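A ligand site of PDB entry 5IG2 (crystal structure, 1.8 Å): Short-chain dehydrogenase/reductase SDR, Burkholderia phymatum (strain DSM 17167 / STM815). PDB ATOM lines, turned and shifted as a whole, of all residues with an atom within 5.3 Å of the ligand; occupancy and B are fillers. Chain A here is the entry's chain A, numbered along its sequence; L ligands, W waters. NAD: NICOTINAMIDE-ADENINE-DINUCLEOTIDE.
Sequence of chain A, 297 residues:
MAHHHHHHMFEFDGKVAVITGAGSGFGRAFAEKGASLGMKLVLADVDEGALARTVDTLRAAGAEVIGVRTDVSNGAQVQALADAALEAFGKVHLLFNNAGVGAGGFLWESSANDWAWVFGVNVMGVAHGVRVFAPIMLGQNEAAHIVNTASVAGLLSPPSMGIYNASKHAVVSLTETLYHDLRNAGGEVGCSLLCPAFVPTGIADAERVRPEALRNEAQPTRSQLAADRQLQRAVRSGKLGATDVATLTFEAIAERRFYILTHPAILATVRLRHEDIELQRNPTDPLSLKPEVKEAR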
ATOM      1  N   GLY A  21      29.607 -19.020 -17.052  1.00  0.00           N
ATOM      2  CA  GLY A  21      29.335 -17.611 -17.308  1.00  0.00           C
ATOM      3  C   GLY A  21      28.198 -17.071 -16.464  1.00  0.00           C
ATOM      4  O   GLY A  21      27.491 -16.155 -16.900  1.00  0.00           O
ATOM      5  N   ALA A  22      28.011 -17.612 -15.258  1.00  0.00           N
ATOM      6  CA  ALA A  22      26.851 -17.257 -14.442  1.00  0.00           C
ATOM      7  C   ALA A  22      26.945 -15.863 -13.803  1.00  0.00           C
ATOM      8  O   ALA A  22      25.967 -15.401 -13.214  1.00  0.00           O
ATOM      9  CB  ALA A  22      26.648 -18.304 -13.335  1.00  0.00           C
ATOM     10  N   GLY A  23      28.091 -15.192 -13.891  1.00  0.00           N
ATOM     11  CA  GLY A  23      28.187 -13.918 -13.228  1.00  0.00           C
ATOM     12  C   GLY A  23      27.546 -12.741 -13.948  1.00  0.00           C
ATOM     13  O   GLY A  23      27.549 -11.635 -13.400  1.00  0.00           O
ATOM     14  N   SER A  24      26.969 -12.956 -15.136  1.00  0.00           N
ATOM     15  CA  SER A  24      26.535 -11.867 -15.995  1.00  0.00           C
ATOM     16  C   SER A  24      25.606 -12.416 -17.071  1.00  0.00           C
ATOM     17  O   SER A  24      25.529 -13.620 -17.286  1.00  0.00           O
ATOM     18  CB  SER A  24      27.735 -11.152 -16.637  1.00  0.00           C
ATOM     19  OG  SER A  24      27.353 -10.012 -17.381  1.00  0.00           O
ATOM     20  N   GLY A  25      24.875 -11.501 -17.720  1.00  0.00           N
ATOM     21  CA  GLY A  25      24.277 -11.802 -19.015  1.00  0.00           C
ATOM     22  C   GLY A  25      23.357 -13.006 -19.012  1.00  0.00           C
ATOM     23  O   GLY A  25      22.522 -13.184 -18.114  1.00  0.00           O
ATOM     24  N   PHE A  26      23.507 -13.857 -20.036  1.00  0.00           N
ATOM     25  CA  PHE A  26      22.636 -15.021 -20.175  1.00  0.00           C
ATOM     26  C   PHE A  26      22.755 -15.950 -18.971  1.00  0.00           C
ATOM     27  O   PHE A  26      21.765 -16.537 -18.527  1.00  0.00           O
ATOM     28  CB  PHE A  26      22.948 -15.816 -21.453  1.00  0.00           C
ATOM     29  CG  PHE A  26      22.761 -15.054 -22.740  1.00  0.00           C
ATOM     30  CD1 PHE A  26      21.980 -13.909 -22.795  1.00  0.00           C
ATOM     31  CD2 PHE A  26      23.368 -15.489 -23.908  1.00  0.00           C
ATOM     32  CE1 PHE A  26      21.819 -13.217 -23.989  1.00  0.00           C
ATOM     33  CE2 PHE A  26      23.227 -14.802 -25.111  1.00  0.00           C
ATOM     34  CZ  PHE A  26      22.452 -13.667 -25.158  1.00  0.00           C
ATOM     35  N   GLY A  27      23.975 -16.116 -18.460  1.00  0.00           N
ATOM     36  CA  GLY A  27      24.181 -17.081 -17.385  1.00  0.00           C
ATOM     37  C   GLY A  27      23.445 -16.701 -16.119  1.00  0.00           C
ATOM     38  O   GLY A  27      22.809 -17.537 -15.472  1.00  0.00           O
ATOM     39  N   ALA A  44      29.165 -20.983 -12.090  1.00  0.00           N
ATOM     40  CA  ALA A  44      30.592 -20.954 -12.371  1.00  0.00           C
ATOM     41  C   ALA A  44      30.939 -19.770 -13.251  1.00  0.00           C
ATOM     42  O   ALA A  44      30.215 -19.461 -14.211  1.00  0.00           O
ATOM     43  CB  ALA A  44      31.068 -22.261 -13.036  1.00  0.00           C
ATOM     44  N   ASP A  45      32.033 -19.092 -12.914  1.00  0.00           N
ATOM     45  CA  ASP A  45      32.527 -17.941 -13.659  1.00  0.00           C
ATOM     46  C   ASP A  45      33.994 -17.739 -13.285  1.00  0.00           C
ATOM     47  O   ASP A  45      34.428 -18.133 -12.200  1.00  0.00           O
ATOM     48  CB  ASP A  45      31.728 -16.673 -13.361  1.00  0.00           C
ATOM     49  CG  ASP A  45      31.726 -15.693 -14.517  1.00  0.00           C
ATOM     50  OD1 ASP A  45      32.802 -15.117 -14.813  1.00  0.00           O
ATOM     51  OD2 ASP A  45      30.639 -15.484 -15.132  1.00  0.00           O
ATOM     52  N   VAL A  46      34.745 -17.140 -14.202  1.00  0.00           N
ATOM     53  CA  VAL A  46      36.118 -16.787 -13.880  1.00  0.00           C
ATOM     54  C   VAL A  46      36.176 -15.429 -13.180  1.00  0.00           C
ATOM     55  O   VAL A  46      37.140 -15.140 -12.468  1.00  0.00           O
ATOM     56  CB  VAL A  46      36.993 -16.800 -15.145  1.00  0.00           C
ATOM     57  CG1 VAL A  46      36.764 -15.522 -15.966  1.00  0.00           C
ATOM     58  CG2 VAL A  46      38.478 -16.979 -14.763  1.00  0.00           C
ATOM     59  N   ASP A  47      35.143 -14.600 -13.350  1.00  0.00           N
ATOM     60  CA  ASP A  47      35.096 -13.289 -12.730  1.00  0.00           C
ATOM     61  C   ASP A  47      34.632 -13.478 -11.283  1.00  0.00           C
ATOM     62  O   ASP A  47      33.440 -13.671 -11.019  1.00  0.00           O
ATOM     63  CB  ASP A  47      34.157 -12.386 -13.536  1.00  0.00           C
ATOM     64  CG  ASP A  47      34.140 -10.958 -13.045  1.00  0.00           C
ATOM     65  OD1 ASP A  47      34.495 -10.687 -11.864  1.00  0.00           O
ATOM     66  OD2 ASP A  47      33.756 -10.096 -13.864  1.00  0.00           O
ATOM     67  N   ALA A  50      31.901 -10.904  -9.953  1.00  0.00           N
ATOM     68  CA  ALA A  50      30.584 -11.096 -10.551  1.00  0.00           C
ATOM     69  C   ALA A  50      29.941 -12.365 -10.044  1.00  0.00           C
ATOM     70  O   ALA A  50      28.733 -12.386  -9.751  1.00  0.00           O
ATOM     71  CB  ALA A  50      30.685 -11.148 -12.079  1.00  0.00           C
ATOM     72  N   THR A  70      35.641 -20.747 -11.722  1.00  0.00           N
ATOM     73  CA  THR A  70      36.021 -21.726 -12.738  1.00  0.00           C
ATOM     74  C   THR A  70      36.440 -20.987 -14.004  1.00  0.00           C
ATOM     75  O   THR A  70      35.674 -20.179 -14.532  1.00  0.00           O
ATOM     76  CB  THR A  70      34.847 -22.663 -13.047  1.00  0.00           C
ATOM     77  OG1 THR A  70      34.380 -23.271 -11.844  1.00  0.00           O
ATOM     78  CG2 THR A  70      35.257 -23.759 -14.058  1.00  0.00           C
ATOM     79  N   ASP A  71      37.655 -21.285 -14.483  1.00  0.00           N
ATOM     80  CA  ASP A  71      38.085 -20.909 -15.828  1.00  0.00           C
ATOM     81  C   ASP A  71      37.755 -22.092 -16.725  1.00  0.00           C
ATOM     82  O   ASP A  71      38.438 -23.123 -16.701  1.00  0.00           O
ATOM     83  CB  ASP A  71      39.580 -20.575 -15.809  1.00  0.00           C
ATOM     84  CG  ASP A  71      40.177 -20.368 -17.197  1.00  0.00           C
ATOM     85  OD1 ASP A  71      39.432 -20.341 -18.208  1.00  0.00           O
ATOM     86  OD2 ASP A  71      41.421 -20.203 -17.270  1.00  0.00           O
ATOM     87  N   VAL A  72      36.691 -21.959 -17.533  1.00  0.00           N
ATOM     88  CA  VAL A  72      36.217 -23.072 -18.340  1.00  0.00           C
ATOM     89  C   VAL A  72      37.227 -23.520 -19.375  1.00  0.00           C
ATOM     90  O   VAL A  72      37.117 -24.636 -19.900  1.00  0.00           O
ATOM     91  CB  VAL A  72      34.864 -22.737 -19.016  1.00  0.00           C
ATOM     92  CG1 VAL A  72      33.777 -22.472 -17.987  1.00  0.00           C
ATOM     93  CG2 VAL A  72      35.015 -21.554 -19.969  1.00  0.00           C
ATOM     94  N   SER A  73      38.215 -22.690 -19.709  1.00  0.00           N
ATOM     95  CA  SER A  73      39.231 -23.155 -20.656  1.00  0.00           C
ATOM     96  C   SER A  73      40.160 -24.201 -20.037  1.00  0.00           C
ATOM     97  O   SER A  73      40.928 -24.848 -20.772  1.00  0.00           O
ATOM     98  CB  SER A  73      40.059 -21.972 -21.191  1.00  0.00           C
ATOM     99  OG  SER A  73      40.924 -21.446 -20.196  1.00  0.00           O
ATOM    100  N   ASN A  98      28.037 -21.953 -21.326  1.00  0.00           N
ATOM    101  CA  ASN A  98      27.559 -20.654 -21.762  1.00  0.00           C
ATOM    102  C   ASN A  98      28.620 -19.561 -21.740  1.00  0.00           C
ATOM    103  O   ASN A  98      28.500 -18.599 -22.502  1.00  0.00           O
ATOM    104  CB  ASN A  98      26.373 -20.243 -20.878  1.00  0.00           C
ATOM    105  CG  ASN A  98      25.980 -18.792 -21.060  1.00  0.00           C
ATOM    106  OD1 ASN A  98      25.351 -18.405 -22.073  1.00  0.00           O
ATOM    107  ND2 ASN A  98      26.328 -17.967 -20.072  1.00  0.00           N
ATOM    108  N   ALA A  99      29.659 -19.686 -20.915  1.00  0.00           N
ATOM    109  CA  ALA A  99      30.718 -18.685 -20.894  1.00  0.00           C
ATOM    110  C   ALA A  99      31.271 -18.441 -22.288  1.00  0.00           C
ATOM    111  O   ALA A  99      31.460 -19.382 -23.074  1.00  0.00           O
ATOM    112  CB  ALA A  99      31.842 -19.133 -19.947  1.00  0.00           C
ATOM    113  N   GLY A 100      31.524 -17.169 -22.605  1.00  0.00           N
ATOM    114  CA  GLY A 100      32.084 -16.828 -23.906  1.00  0.00           C
ATOM    115  C   GLY A 100      32.757 -15.479 -23.896  1.00  0.00           C
ATOM    116  O   GLY A 100      32.501 -14.637 -23.029  1.00  0.00           O
ATOM    117  N   VAL A 101      33.658 -15.292 -24.862  1.00  0.00           N
ATOM    118  CA  VAL A 101      34.398 -14.056 -25.039  1.00  0.00           C
ATOM    119  C   VAL A 101      34.473 -13.792 -26.536  1.00  0.00           C
ATOM    120  O   VAL A 101      34.112 -14.629 -27.362  1.00  0.00           O
ATOM    121  CB  VAL A 101      35.816 -14.114 -24.420  1.00  0.00           C
ATOM    122  CG1 VAL A 101      35.753 -14.367 -22.904  1.00  0.00           C
ATOM    123  CG2 VAL A 101      36.661 -15.166 -25.107  1.00  0.00           C
ATOM    124  N   VAL A 121      38.089 -20.322 -24.462  1.00  0.00           N
ATOM    125  CA  VAL A 121      36.817 -20.162 -23.754  1.00  0.00           C
ATOM    126  C   VAL A 121      35.671 -20.747 -24.572  1.00  0.00           C
ATOM    127  O   VAL A 121      34.891 -21.573 -24.066  1.00  0.00           O
ATOM    128  CB  VAL A 121      36.551 -18.688 -23.416  1.00  0.00           C
ATOM    129  CG1 VAL A 121      35.183 -18.533 -22.715  1.00  0.00           C
ATOM    130  CG2 VAL A 121      37.670 -18.121 -22.548  1.00  0.00           C
ATOM    131  N   ASN A 122      35.523 -20.313 -25.825  1.00  0.00           N
ATOM    132  CA  ASN A 122      34.274 -20.560 -26.561  1.00  0.00           C
ATOM    133  C   ASN A 122      34.169 -21.989 -27.057  1.00  0.00           C
ATOM    134  O   ASN A 122      33.057 -22.496 -27.184  1.00  0.00           O
ATOM    135  CB  ASN A 122      34.144 -19.618 -27.766  1.00  0.00           C
ATOM    136  CG  ASN A 122      33.954 -18.166 -27.362  1.00  0.00           C
ATOM    137  OD1 ASN A 122      34.041 -17.812 -26.192  1.00  0.00           O
ATOM    138  ND2 ASN A 122      33.709 -17.305 -28.360  1.00  0.00           N
ATOM    139  N   THR A 149      25.840 -22.558 -25.673  1.00  0.00           N
ATOM    140  CA  THR A 149      25.534 -21.235 -26.230  1.00  0.00           C
ATOM    141  C   THR A 149      26.466 -20.986 -27.410  1.00  0.00           C
ATOM    142  O   THR A 149      27.673 -20.783 -27.224  1.00  0.00           O
ATOM    143  CB  THR A 149      25.657 -20.120 -25.201  1.00  0.00           C
ATOM    144  OG1 THR A 149      24.829 -20.371 -24.056  1.00  0.00           O
ATOM    145  CG2 THR A 149      25.215 -18.818 -25.831  1.00  0.00           C
ATOM    146  N   ALA A 150      25.910 -20.992 -28.616  1.00  0.00           N
ATOM    147  CA  ALA A 150      26.681 -20.537 -29.761  1.00  0.00           C
ATOM    148  C   ALA A 150      26.346 -19.068 -29.967  1.00  0.00           C
ATOM    149  O   ALA A 150      26.595 -18.244 -29.080  1.00  0.00           O
ATOM    150  CB  ALA A 150      26.374 -21.371 -31.012  1.00  0.00           C
ATOM    151  N   SER A 151      25.747 -18.750 -31.119  1.00  0.00           N
ATOM    152  CA  SER A 151      25.401 -17.383 -31.511  1.00  0.00           C
ATOM    153  C   SER A 151      24.882 -17.442 -32.944  1.00  0.00           C
ATOM    154  O   SER A 151      25.152 -18.433 -33.641  1.00  0.00           O
ATOM    155  CB  SER A 151      26.621 -16.458 -31.422  1.00  0.00           C
ATOM    156  OG  SER A 151      26.411 -15.267 -32.125  1.00  0.00           O
ATOM    157  N   VAL A 152      24.169 -16.418 -33.417  1.00  0.00           N
ATOM    158  CA  VAL A 152      23.913 -16.378 -34.858  1.00  0.00           C
ATOM    159  C   VAL A 152      25.229 -16.275 -35.609  1.00  0.00           C
ATOM    160  O   VAL A 152      25.294 -16.615 -36.796  1.00  0.00           O
ATOM    161  CB  VAL A 152      22.959 -15.245 -35.277  1.00  0.00           C
ATOM    162  CG1 VAL A 152      21.598 -15.401 -34.583  1.00  0.00           C
ATOM    163  CG2 VAL A 152      23.581 -13.887 -35.022  1.00  0.00           C
ATOM    164  N   TYR A 164      35.791 -14.969 -33.551  1.00  0.00           N
ATOM    165  CA  TYR A 164      34.554 -15.256 -32.841  1.00  0.00           C
ATOM    166  C   TYR A 164      33.635 -16.128 -33.686  1.00  0.00           C
ATOM    167  O   TYR A 164      33.125 -17.150 -33.225  1.00  0.00           O
ATOM    168  CB  TYR A 164      33.864 -13.935 -32.487  1.00  0.00           C
ATOM    169  CG  TYR A 164      32.617 -14.068 -31.661  1.00  0.00           C
ATOM    170  CD1 TYR A 164      32.693 -14.329 -30.308  1.00  0.00           C
ATOM    171  CD2 TYR A 164      31.352 -13.914 -32.229  1.00  0.00           C
ATOM    172  CE1 TYR A 164      31.565 -14.449 -29.537  1.00  0.00           C
ATOM    173  CE2 TYR A 164      30.196 -14.029 -31.455  1.00  0.00           C
ATOM    174  CZ  TYR A 164      30.314 -14.298 -30.106  1.00  0.00           C
ATOM    175  OH  TYR A 164      29.203 -14.416 -29.308  1.00  0.00           O
ATOM    176  N   LYS A 168      32.249 -19.949 -32.892  1.00  0.00           N
ATOM    177  CA  LYS A 168      30.828 -20.258 -32.746  1.00  0.00           C
ATOM    178  C   LYS A 168      30.354 -21.275 -33.775  1.00  0.00           C
ATOM    179  O   LYS A 168      29.488 -22.098 -33.466  1.00  0.00           O
ATOM    180  CB  LYS A 168      30.008 -18.964 -32.809  1.00  0.00           C
ATOM    181  CG  LYS A 168      30.246 -18.036 -31.612  1.00  0.00           C
ATOM    182  CD  LYS A 168      30.014 -18.776 -30.292  1.00  0.00           C
ATOM    183  CE  LYS A 168      29.960 -17.805 -29.125  1.00  0.00           C
ATOM    184  NZ  LYS A 168      29.521 -18.467 -27.846  1.00  0.00           N
ATOM    185  N   PRO A 196      21.568 -16.930 -30.194  1.00  0.00           N
ATOM    186  CA  PRO A 196      20.955 -15.609 -30.132  1.00  0.00           C
ATOM    187  C   PRO A 196      21.642 -14.599 -31.048  1.00  0.00           C
ATOM    188  O   PRO A 196      22.809 -14.749 -31.426  1.00  0.00           O
ATOM    189  CB  PRO A 196      21.123 -15.198 -28.657  1.00  0.00           C
ATOM    190  CG  PRO A 196      21.610 -16.462 -27.938  1.00  0.00           C
ATOM    191  CD  PRO A 196      22.351 -17.228 -28.984  1.00  0.00           C
ATOM    192  N   ALA A 197      20.869 -13.594 -31.445  1.00  0.00           N
ATOM    193  CA  ALA A 197      21.420 -12.369 -31.999  1.00  0.00           C
ATOM    194  C   ALA A 197      21.766 -11.423 -30.840  1.00  0.00           C
ATOM    195  O   ALA A 197      21.710 -11.816 -29.666  1.00  0.00           O
ATOM    196  CB  ALA A 197      20.446 -11.739 -32.999  1.00  0.00           C
ATOM    197  N   PHE A 198      22.116 -10.177 -31.153  1.00  0.00           N
ATOM    198  CA  PHE A 198      22.695  -9.284 -30.149  1.00  0.00           C
ATOM    199  C   PHE A 198      21.715  -9.009 -29.014  1.00  0.00           C
ATOM    200  O   PHE A 198      20.537  -8.702 -29.248  1.00  0.00           O
ATOM    201  CB  PHE A 198      23.146  -7.963 -30.781  1.00  0.00           C
ATOM    202  CG  PHE A 198      24.093  -8.123 -31.935  1.00  0.00           C
ATOM    203  CD1 PHE A 198      25.419  -8.447 -31.712  1.00  0.00           C
ATOM    204  CD2 PHE A 198      23.644  -7.957 -33.237  1.00  0.00           C
ATOM    205  CE1 PHE A 198      26.284  -8.599 -32.775  1.00  0.00           C
ATOM    206  CE2 PHE A 198      24.511  -8.100 -34.303  1.00  0.00           C
ATOM    207  CZ  PHE A 198      25.831  -8.421 -34.072  1.00  0.00           C
ATOM    208  N   VAL A 199      22.208  -9.091 -27.780  1.00  0.00           N
ATOM    209  CA  VAL A 199      21.434  -8.847 -26.569  1.00  0.00           C
ATOM    210  C   VAL A 199      22.270  -7.960 -25.650  1.00  0.00           C
ATOM    211  O   VAL A 199      23.471  -8.212 -25.492  1.00  0.00           O
ATOM    212  CB  VAL A 199      21.057 -10.159 -25.869  1.00  0.00           C
ATOM    213  CG1 VAL A 199      20.292  -9.889 -24.554  1.00  0.00           C
ATOM    214  CG2 VAL A 199      20.220 -11.056 -26.786  1.00  0.00           C
ATOM    215  N   THR A 201      24.223  -7.351 -22.958  1.00  0.00           N
ATOM    216  CA  THR A 201      24.861  -8.064 -21.856  1.00  0.00           C
ATOM    217  C   THR A 201      26.246  -7.430 -21.683  1.00  0.00           C
ATOM    218  O   THR A 201      26.499  -6.307 -22.152  1.00  0.00           O
ATOM    219  CB  THR A 201      24.976  -9.566 -22.134  1.00  0.00           C
ATOM    220  OG1 THR A 201      25.881  -9.752 -23.234  1.00  0.00           O
ATOM    221  CG2 THR A 201      23.614 -10.153 -22.496  1.00  0.00           C
ATOM    222  N   GLY A 202      27.161  -8.163 -21.050  1.00  0.00           N
ATOM    223  CA  GLY A 202      28.537  -7.717 -20.907  1.00  0.00           C
ATOM    224  C   GLY A 202      29.470  -8.202 -21.990  1.00  0.00           C
ATOM    225  O   GLY A 202      30.688  -7.972 -21.882  1.00  0.00           O
ATOM    226  N   ILE A 203      28.952  -8.846 -23.046  1.00  0.00           N
ATOM    227  CA  ILE A 203      29.816  -9.570 -23.970  1.00  0.00           C
ATOM    228  C   ILE A 203      30.764  -8.635 -24.703  1.00  0.00           C
ATOM    229  O   ILE A 203      31.894  -9.009 -25.044  1.00  0.00           O
ATOM    230  CB  ILE A 203      28.961 -10.413 -24.943  1.00  0.00           C
ATOM    231  CG1 ILE A 203      29.831 -11.359 -25.772  1.00  0.00           C
ATOM    232  CG2 ILE A 203      28.145  -9.509 -25.874  1.00  0.00           C
ATOM    233  CD1 ILE A 203      30.571 -12.418 -24.931  1.00  0.00           C
ATOM    234  N   ARG A 208      37.612  -7.601 -20.131  1.00  0.00           N
ATOM    235  CA  ARG A 208      37.767  -7.522 -18.686  1.00  0.00           C
ATOM    236  C   ARG A 208      38.223  -8.851 -18.077  1.00  0.00           C
ATOM    237  O   ARG A 208      38.781  -8.852 -16.971  1.00  0.00           O
ATOM    238  CB  ARG A 208      36.454  -7.076 -18.027  1.00  0.00           C
ATOM    239  CG  ARG A 208      35.337  -8.151 -17.993  1.00  0.00           C
ATOM    240  CD  ARG A 208      34.039  -7.592 -17.382  1.00  0.00           C
ATOM    241  NE  ARG A 208      32.914  -8.537 -17.380  1.00  0.00           N
ATOM    242  CZ  ARG A 208      32.181  -8.841 -18.454  1.00  0.00           C
ATOM    243  NH1 ARG A 208      32.454  -8.311 -19.641  1.00  0.00           N
ATOM    244  NH2 ARG A 208      31.162  -9.703 -18.341  1.00  0.00           N
ATOM    245  N   VAL A 209      38.015  -9.968 -18.768  1.00  0.00           N
ATOM    246  CA  VAL A 209      38.435 -11.250 -18.226  1.00  0.00           C
ATOM    247  C   VAL A 209      39.452 -11.936 -19.134  1.00  0.00           C
ATOM    248  O   VAL A 209      39.609 -13.150 -19.062  1.00  0.00           O
ATOM    249  CB  VAL A 209      37.233 -12.181 -17.963  1.00  0.00           C
ATOM    250  CG1 VAL A 209      36.416 -11.670 -16.733  1.00  0.00           C
ATOM    251  CG2 VAL A 209      36.362 -12.330 -19.227  1.00  0.00           C
ATOM    252  N   VAL A 235      25.319  -4.702 -29.520  1.00  0.00           N
ATOM    253  CA  VAL A 235      24.917  -5.277 -28.237  1.00  0.00           C
ATOM    254  C   VAL A 235      23.944  -4.353 -27.520  1.00  0.00           C
ATOM    255  O   VAL A 235      22.856  -4.785 -27.106  1.00  0.00           O
ATOM    256  CB  VAL A 235      26.165  -5.577 -27.393  1.00  0.00           C
ATOM    257  CG1 VAL A 235      25.787  -5.810 -25.945  1.00  0.00           C
ATOM    258  CG2 VAL A 235      26.905  -6.807 -27.955  1.00  0.00           C
HETATM  259  PA  NAD L   1      28.530 -11.624 -20.515  1.00  0.00           P
HETATM  260  O1A NAD L   1      29.824 -10.935 -20.662  1.00  0.00           O
HETATM  261  O2A NAD L   1      27.440 -10.759 -19.897  1.00  0.00           O
HETATM  262  O5B NAD L   1      28.659 -13.009 -19.701  1.00  0.00           O
HETATM  263  C5B NAD L   1      29.687 -13.951 -20.099  1.00  0.00           C
HETATM  264  C4B NAD L   1      30.342 -14.434 -18.830  1.00  0.00           C
HETATM  265  O4B NAD L   1      31.341 -15.436 -19.128  1.00  0.00           O
HETATM  266  C3B NAD L   1      31.044 -13.345 -18.008  1.00  0.00           C
HETATM  267  O3B NAD L   1      30.496 -13.315 -16.689  1.00  0.00           O
HETATM  268  C2B NAD L   1      32.518 -13.766 -18.044  1.00  0.00           C
HETATM  269  O2B NAD L   1      33.240 -13.431 -16.858  1.00  0.00           O
HETATM  270  C1B NAD L   1      32.392 -15.271 -18.209  1.00  0.00           C
HETATM  271  N9A NAD L   1      33.589 -15.922 -18.728  1.00  0.00           N
HETATM  272  C8A NAD L   1      34.443 -15.449 -19.685  1.00  0.00           C
HETATM  273  N7A NAD L   1      35.522 -16.175 -19.846  1.00  0.00           N
HETATM  274  C5A NAD L   1      35.363 -17.211 -18.941  1.00  0.00           C
HETATM  275  C6A NAD L   1      36.169 -18.314 -18.607  1.00  0.00           C
HETATM  276  N6A NAD L   1      37.374 -18.549 -19.152  1.00  0.00           N
HETATM  277  N1A NAD L   1      35.717 -19.162 -17.660  1.00  0.00           N
HETATM  278  C2A NAD L   1      34.542 -18.905 -17.073  1.00  0.00           C
HETATM  279  N3A NAD L   1      33.697 -17.890 -17.295  1.00  0.00           N
HETATM  280  C4A NAD L   1      34.170 -17.078 -18.255  1.00  0.00           C
HETATM  281  O3  NAD L   1      28.060 -12.066 -21.981  1.00  0.00           O
HETATM  282  PN  NAD L   1      26.823 -12.953 -22.483  1.00  0.00           P
HETATM  283  O1N NAD L   1      25.941 -13.267 -21.336  1.00  0.00           O
HETATM  284  O2N NAD L   1      26.258 -12.299 -23.681  1.00  0.00           O
HETATM  285  O5D NAD L   1      27.612 -14.265 -22.932  1.00  0.00           O
HETATM  286  C5D NAD L   1      27.056 -15.587 -22.782  1.00  0.00           C
HETATM  287  C4D NAD L   1      27.227 -16.351 -24.074  1.00  0.00           C
HETATM  288  O4D NAD L   1      26.320 -15.833 -25.068  1.00  0.00           O
HETATM  289  C3D NAD L   1      28.629 -16.292 -24.694  1.00  0.00           C
HETATM  290  O3D NAD L   1      29.052 -17.593 -25.130  1.00  0.00           O
HETATM  291  C2D NAD L   1      28.441 -15.327 -25.873  1.00  0.00           C
HETATM  292  O2D NAD L   1      29.411 -15.512 -26.910  1.00  0.00           O
HETATM  293  C1D NAD L   1      27.024 -15.715 -26.270  1.00  0.00           C
HETATM  294  N1N NAD L   1      26.266 -14.738 -27.191  1.00  0.00           N
HETATM  295  C2N NAD L   1      26.066 -13.483 -26.751  1.00  0.00           C
HETATM  296  C3N NAD L   1      25.371 -12.573 -27.527  1.00  0.00           C
HETATM  297  C7N NAD L   1      24.971 -11.224 -27.022  1.00  0.00           C
HETATM  298  O7N NAD L   1      24.648 -10.351 -27.837  1.00  0.00           O
HETATM  299  N7N NAD L   1      25.103 -10.989 -25.719  1.00  0.00           N
HETATM  300  C4N NAD L   1      24.872 -13.003 -28.759  1.00  0.00           C
HETATM  301  C5N NAD L   1      25.074 -14.305 -29.171  1.00  0.00           C
HETATM  302  C6N NAD L   1      25.780 -15.172 -28.374  1.00  0.00           C
HETATM  303  O   HOH W   1      38.292 -15.401 -20.318  1.00  0.00           O
HETATM  304  O   HOH W   2      31.291 -10.812 -15.599  1.00  0.00           O
HETATM  305  O   HOH W   3      26.588 -15.314 -19.476  1.00  0.00           O
HETATM  306  O   HOH W   4      29.502 -20.822 -24.595  1.00  0.00           O
HETATM  307  O   HOH W   5      32.712 -12.150 -21.372  1.00  0.00           O
HETATM  308  O   HOH W   6      40.246 -17.613 -20.655  1.00  0.00           O
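O2A of the ligand is in hydrogen-bond range of N of Gly 202 (2.9 Å).
The side-chain carboxylate (OD2) of Asp 45 lies within hydrogen-bond range of an oxygen (O3B) of the ligand, 2.7 Å away.
The backbone NH (N) of Val 199 is in hydrogen-bond range of an oxygen (O7N) of the ligand (2.7 Å).
The backbone NH (N) of Gly 25 sits at hydrogen-bond distance from an oxygen (O2A) of the ligand (3.4 Å).
A nitrogen (N6A) of the ligand is in hydrogen-bond range of the side-chain carboxylate (OD1) of Asp 71 (2.9 Å).
The guanidinium group (NH2) of Arg 208 is in salt-bridge range of an oxygen (O1A) of the ligand (2.9 Å).
O2A of the ligand sits at hydrogen-bond distance from OG of Ser 24, at 2.6 Å.
The backbone NH of Val 72 lies within hydrogen-bond range of a nitrogen (N1A) of the ligand (3.0 Å).
N7N of the ligand lies within hydrogen-bond range of O of Val 199 (3.2 Å).
The backbone carbonyl oxygen (O) of Asn 98 lies within hydrogen-bond range of an oxygen (O3D) of the ligand (2.9 Å).
The backbone NH (N) of Ile 203 lies within hydrogen-bond range of an oxygen (O1A) of the ligand (3.3 Å).
The side-chain hydroxyl (OG1) of Thr 201 sits at hydrogen-bond distance from an oxygen (O2N) of the ligand, at 2.6 Å.
An oxygen (O2D) of the ligand is in hydrogen-bond range of the side-chain hydroxyl (OH) of Tyr 164 (2.6 Å).
The backbone NH of Val 46 sits at hydrogen-bond distance from a nitrogen (N3A) of the ligand (3.4 Å).
An oxygen (O1N) of the ligand is in hydrogen-bond range of the backbone NH of Phe 26.
The side-chain amino group (NZ) of Lys 168 lies within hydrogen-bond range of an oxygen (O3D) of the ligand (2.9 Å).
Water W2 lies within hydrogen-bond range of O3B of the ligand, NH2 of Arg 208 and OD2 of Asp 47.
Water W1 bridges the backbone carbonyl oxygen of Val 209 (2.9 Å) and a nitrogen (N7A) of the ligand (2.9 Å).
Water W5 lies within hydrogen-bond range of the backbone carbonyl oxygen of Gly 100 (3.0 Å) and an oxygen (O1A) of the ligand (3.2 Å).
The backbone carbonyl oxygen of Pro 196 sits at hydrogen-bond distance from the backbone NH of Val 152.
N of Gly 21 sits at hydrogen-bond distance from O of Ala 44 (2.9 Å).
The backbone NH of Thr 70 lies within hydrogen-bond range of the backbone carbonyl oxygen of Asp 45 (2.9 Å).
The side-chain carboxylate of Asp 45 lies within hydrogen-bond range of the backbone NH of Asp 47, at 2.8 Å.
ND2 of Asn 98 sits close to N of Gly 27.
The side-chain carboxylate of Asp 71 is in hydrogen-bond range of the side-chain hydroxyl of Ser 73, at 2.7 Å.
The side-chain carboxylate (OD1) of Asp 47 lies within hydrogen-bond range of the backbone NH (N) of Ala 50 (3.2 Å).
The backbone NH (N) of Ile 203 is in hydrogen-bond range of the side-chain hydroxyl (OG1) of Thr 201.
The backbone carbonyl oxygen (O) of Thr 70 lies close to a nitrogen (N1A) of the ligand, at 3.3 Å.
Merely in contact with the ligand: Phe 198 (3.2 Å), Pro 196 (3.2 Å), Ala 150 (3.3 Å), Thr 149 (3.3 Å), Gly 100 (3.4 Å), Ser 151 (3.4 Å), Val 121 (3.4 Å), Ala 99 (3.5 Å), Gly 21 (3.5 Å), Ala 197 (3.5 Å), Val 101 (3.6 Å), Asp 47 (3.6 Å) and Val 209 (3.6 Å).
29 residues have an atom within 4 Å of the ligand: Gly 21, Ser 24, Gly 25, Phe 26, Asp 45, Val 46, Asp 47, Thr 70, Asp 71, Val 72, Asn 98, Ala 99, Gly 100, Val 101, Val 121, Thr 149, Ala 150, Ser 151, Tyr 164, Lys 168, Pro 196, Ala 197, Phe 198, Val 199, Thr 201, Gly 202, Ile 203, Arg 208 and Val 209.
Along chain A the residues within 4 Å of the ligand span positions 21 to 209.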
